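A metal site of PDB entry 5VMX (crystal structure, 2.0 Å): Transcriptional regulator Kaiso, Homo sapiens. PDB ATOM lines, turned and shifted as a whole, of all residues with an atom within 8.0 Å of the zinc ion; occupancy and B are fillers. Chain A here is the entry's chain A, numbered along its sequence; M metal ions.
SG of Cys 82 lies close to N of Ala 84, at 3.4 Å. The backbone NH of Cys 82 sits at hydrogen-bond distance from the backbone carbonyl oxygen of Lys 87 (2.8 Å). SG of Cys 85 sits close to N of Lys 87, 3.6 Å away.
Of the 16 residues printed, 4 come within 4 Å of the zinc ion. The nearest printed residue that does not touch the zinc ion is Ala 84 (4.4 Å).
The zinc ion is bound by a ring nitrogen (NE2) of His 98 (2.0 Å), a ring nitrogen (NE2) of His 103 (2.1 Å), the side-chain sulfur (SG) of Cys 82 (2.3 Å) and the side-chain sulfur (SG) of Cys 85 (2.3 Å).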
ATOM      1  N   GLN A  81      -6.118  -7.233   6.231  1.00  0.00           N
ATOM      2  CA  GLN A  81      -6.952  -7.485   7.391  1.00  0.00           C
ATOM      3  C   GLN A  81      -7.943  -8.635   7.189  1.00  0.00           C
ATOM      4  O   GLN A  81      -8.719  -8.622   6.233  1.00  0.00           O
ATOM      5  CB  GLN A  81      -7.710  -6.224   7.808  1.00  0.00           C
ATOM      6  CG  GLN A  81      -8.646  -6.455   9.057  1.00  0.00           C
ATOM      7  CD  GLN A  81      -9.214  -5.150   9.609  1.00  0.00           C
ATOM      8  OE1 GLN A  81      -9.395  -4.198   8.861  1.00  0.00           O
ATOM      9  NE2 GLN A  81      -9.501  -5.102  10.930  1.00  0.00           N
ATOM     10  N   CYS A  82      -7.907  -9.586   8.118  1.00  0.00           N
ATOM     11  CA  CYS A  82      -8.871 -10.682   8.133  1.00  0.00           C
ATOM     12  C   CYS A  82     -10.255 -10.169   8.500  1.00  0.00           C
ATOM     13  O   CYS A  82     -10.452  -9.524   9.543  1.00  0.00           O
ATOM     14  CB  CYS A  82      -8.428 -11.775   9.113  1.00  0.00           C
ATOM     15  SG  CYS A  82      -9.703 -13.058   9.422  1.00  0.00           S
ATOM     16  N   LEU A  83     -11.238 -10.454   7.645  1.00  0.00           N
ATOM     17  CA  LEU A  83     -12.574  -9.902   7.880  1.00  0.00           C
ATOM     18  C   LEU A  83     -13.399 -10.794   8.808  1.00  0.00           C
ATOM     19  O   LEU A  83     -14.472 -10.400   9.220  1.00  0.00           O
ATOM     20  CB  LEU A  83     -13.304  -9.675   6.559  1.00  0.00           C
ATOM     21  CG  LEU A  83     -12.664  -8.591   5.672  1.00  0.00           C
ATOM     22  CD1 LEU A  83     -13.375  -8.450   4.344  1.00  0.00           C
ATOM     23  CD2 LEU A  83     -12.603  -7.248   6.404  1.00  0.00           C
ATOM     24  N   ALA A  84     -12.900 -11.971   9.144  1.00  0.00           N
ATOM     25  CA  ALA A  84     -13.599 -12.879  10.056  1.00  0.00           C
ATOM     26  C   ALA A  84     -13.369 -12.531  11.533  1.00  0.00           C
ATOM     27  O   ALA A  84     -14.269 -12.689  12.340  1.00  0.00           O
ATOM     28  CB  ALA A  84     -13.190 -14.316   9.784  1.00  0.00           C
ATOM     29  N   CYS A  85     -12.177 -12.059  11.886  1.00  0.00           N
ATOM     30  CA  CYS A  85     -11.867 -11.727  13.282  1.00  0.00           C
ATOM     31  C   CYS A  85     -11.216 -10.344  13.490  1.00  0.00           C
ATOM     32  O   CYS A  85     -11.039  -9.900  14.621  1.00  0.00           O
ATOM     33  CB  CYS A  85     -10.956 -12.817  13.871  1.00  0.00           C
ATOM     34  SG  CYS A  85      -9.238 -12.707  13.267  1.00  0.00           S
ATOM     35  N   GLY A  86     -10.836  -9.680  12.400  1.00  0.00           N
ATOM     36  CA  GLY A  86     -10.254  -8.350  12.451  1.00  0.00           C
ATOM     37  C   GLY A  86      -8.736  -8.224  12.537  1.00  0.00           C
ATOM     38  O   GLY A  86      -8.170  -7.079  12.412  1.00  0.00           O
ATOM     39  N   LYS A  87      -8.056  -9.346  12.792  1.00  0.00           N
ATOM     40  CA  LYS A  87      -6.584  -9.318  12.885  1.00  0.00           C
ATOM     41  C   LYS A  87      -5.967  -8.848  11.591  1.00  0.00           C
ATOM     42  O   LYS A  87      -6.474  -9.157  10.507  1.00  0.00           O
ATOM     43  CB  LYS A  87      -5.987 -10.675  13.245  1.00  0.00           C
ATOM     44  CG  LYS A  87      -6.194 -11.077  14.700  1.00  0.00           C
ATOM     45  CD  LYS A  87      -5.326 -12.265  15.091  1.00  0.00           C
ATOM     46  CE  LYS A  87      -5.518 -12.603  16.568  1.00  0.00           C
ATOM     47  NZ  LYS A  87      -6.897 -13.062  16.853  1.00  0.00           N
ATOM     48  N   SER A  88      -4.881  -8.088  11.706  1.00  0.00           N
ATOM     49  CA  SER A  88      -4.197  -7.550  10.514  1.00  0.00           C
ATOM     50  C   SER A  88      -2.775  -8.119  10.373  1.00  0.00           C
ATOM     51  O   SER A  88      -2.132  -8.500  11.368  1.00  0.00           O
ATOM     52  CB  SER A  88      -4.151  -6.022  10.564  1.00  0.00           C
ATOM     53  OG  SER A  88      -5.415  -5.479  10.918  1.00  0.00           O
ATOM     54  N   PHE A  89      -2.279  -8.130   9.140  1.00  0.00           N
ATOM     55  CA  PHE A  89      -1.035  -8.828   8.755  1.00  0.00           C
ATOM     56  C   PHE A  89      -0.251  -7.959   7.787  1.00  0.00           C
ATOM     57  O   PHE A  89      -0.847  -7.138   7.067  1.00  0.00           O
ATOM     58  CB  PHE A  89      -1.355 -10.213   8.125  1.00  0.00           C
ATOM     59  CG  PHE A  89      -2.212 -11.070   9.034  1.00  0.00           C
ATOM     60  CD1 PHE A  89      -1.616 -11.853  10.033  1.00  0.00           C
ATOM     61  CD2 PHE A  89      -3.580 -11.020   8.964  1.00  0.00           C
ATOM     62  CE1 PHE A  89      -2.384 -12.583  10.925  1.00  0.00           C
ATOM     63  CE2 PHE A  89      -4.379 -11.762   9.855  1.00  0.00           C
ATOM     64  CZ  PHE A  89      -3.761 -12.547  10.830  1.00  0.00           C
ATOM     65  N   MET A  95      -1.558 -13.353   6.150  1.00  0.00           N
ATOM     66  CA  MET A  95      -3.015 -13.297   6.122  1.00  0.00           C
ATOM     67  C   MET A  95      -3.618 -14.662   5.669  1.00  0.00           C
ATOM     68  O   MET A  95      -4.533 -15.197   6.295  1.00  0.00           O
ATOM     69  CB  MET A  95      -3.479 -12.153   5.185  1.00  0.00           C
ATOM     70  CG  MET A  95      -5.016 -12.118   4.885  1.00  0.00           C
ATOM     71  SD  MET A  95      -5.637 -13.311   3.630  1.00  0.00           S
ATOM     72  CE  MET A  95      -4.734 -12.780   2.157  1.00  0.00           C
ATOM     73  N   HIS A  98      -3.057 -17.459   8.159  1.00  0.00           N
ATOM     74  CA  HIS A  98      -4.022 -17.240   9.245  1.00  0.00           C
ATOM     75  C   HIS A  98      -5.420 -17.725   8.883  1.00  0.00           C
ATOM     76  O   HIS A  98      -6.026 -18.477   9.625  1.00  0.00           O
ATOM     77  CB  HIS A  98      -4.103 -15.748   9.633  1.00  0.00           C
ATOM     78  CG  HIS A  98      -5.311 -15.415  10.473  1.00  0.00           C
ATOM     79  ND1 HIS A  98      -5.344 -15.615  11.839  1.00  0.00           N
ATOM     80  CD2 HIS A  98      -6.503 -14.891  10.134  1.00  0.00           C
ATOM     81  CE1 HIS A  98      -6.513 -15.226  12.304  1.00  0.00           C
ATOM     82  NE2 HIS A  98      -7.243 -14.788  11.298  1.00  0.00           N
ATOM     83  N   ILE A  99      -5.947 -17.273   7.762  1.00  0.00           N
ATOM     84  CA  ILE A  99      -7.321 -17.619   7.426  1.00  0.00           C
ATOM     85  C   ILE A  99      -7.492 -19.116   7.193  1.00  0.00           C
ATOM     86  O   ILE A  99      -8.493 -19.727   7.636  1.00  0.00           O
ATOM     87  CB  ILE A  99      -7.794 -16.795   6.206  1.00  0.00           C
ATOM     88  CG1 ILE A  99      -7.883 -15.324   6.670  1.00  0.00           C
ATOM     89  CG2 ILE A  99      -9.144 -17.299   5.721  1.00  0.00           C
ATOM     90  CD1 ILE A  99      -8.396 -14.347   5.629  1.00  0.00           C
ATOM     91  N   LYS A 100      -6.502 -19.745   6.558  1.00  0.00           N
ATOM     92  CA  LYS A 100      -6.601 -21.189   6.349  1.00  0.00           C
ATOM     93  C   LYS A 100      -6.507 -21.931   7.678  1.00  0.00           C
ATOM     94  O   LYS A 100      -7.220 -22.892   7.906  1.00  0.00           O
ATOM     95  CB  LYS A 100      -5.526 -21.689   5.379  1.00  0.00           C
ATOM     96  CG  LYS A 100      -5.747 -21.260   3.927  1.00  0.00           C
ATOM     97  CD  LYS A 100      -4.546 -21.690   3.057  1.00  0.00           C
ATOM     98  CE  LYS A 100      -4.705 -21.277   1.598  1.00  0.00           C
ATOM     99  NZ  LYS A 100      -3.538 -21.703   0.730  1.00  0.00           N
ATOM    100  N   VAL A 102      -6.828 -20.786  11.053  1.00  0.00           N
ATOM    101  CA  VAL A 102      -7.728 -20.404  12.132  1.00  0.00           C
ATOM    102  C   VAL A 102      -9.168 -20.480  11.662  1.00  0.00           C
ATOM    103  O   VAL A 102     -10.039 -20.902  12.409  1.00  0.00           O
ATOM    104  CB  VAL A 102      -7.415 -18.965  12.666  1.00  0.00           C
ATOM    105  CG1 VAL A 102      -8.422 -18.535  13.726  1.00  0.00           C
ATOM    106  CG2 VAL A 102      -5.988 -18.890  13.203  1.00  0.00           C
ATOM    107  N   HIS A 103      -9.432 -20.093  10.405  1.00  0.00           N
ATOM    108  CA  HIS A 103     -10.827 -20.049   9.955  1.00  0.00           C
ATOM    109  C   HIS A 103     -11.206 -21.185   8.996  1.00  0.00           C
ATOM    110  O   HIS A 103     -12.370 -21.301   8.606  1.00  0.00           O
ATOM    111  CB  HIS A 103     -11.108 -18.672   9.339  1.00  0.00           C
ATOM    112  CG  HIS A 103     -10.933 -17.539  10.299  1.00  0.00           C
ATOM    113  ND1 HIS A 103     -11.669 -17.439  11.455  1.00  0.00           N
ATOM    114  CD2 HIS A 103     -10.067 -16.494  10.304  1.00  0.00           C
ATOM    115  CE1 HIS A 103     -11.287 -16.357  12.131  1.00  0.00           C
ATOM    116  NE2 HIS A 103     -10.329 -15.768  11.450  1.00  0.00           N
ATOM    117  N   LEU A 113     -12.672 -12.589   1.960  1.00  0.00           N
ATOM    118  CA  LEU A 113     -12.328 -12.910   3.339  1.00  0.00           C
ATOM    119  C   LEU A 113     -11.329 -11.933   3.934  1.00  0.00           C
ATOM    120  O   LEU A 113     -11.021 -11.998   5.116  1.00  0.00           O
ATOM    121  CB  LEU A 113     -11.764 -14.331   3.422  1.00  0.00           C
ATOM    122  CG  LEU A 113     -12.739 -15.380   2.866  1.00  0.00           C
ATOM    123  CD1 LEU A 113     -12.154 -16.782   2.968  1.00  0.00           C
ATOM    124  CD2 LEU A 113     -14.109 -15.309   3.567  1.00  0.00           C
HETATM  125 ZN    ZN M   1      -9.124 -14.031  11.402  1.00  0.00          ZN
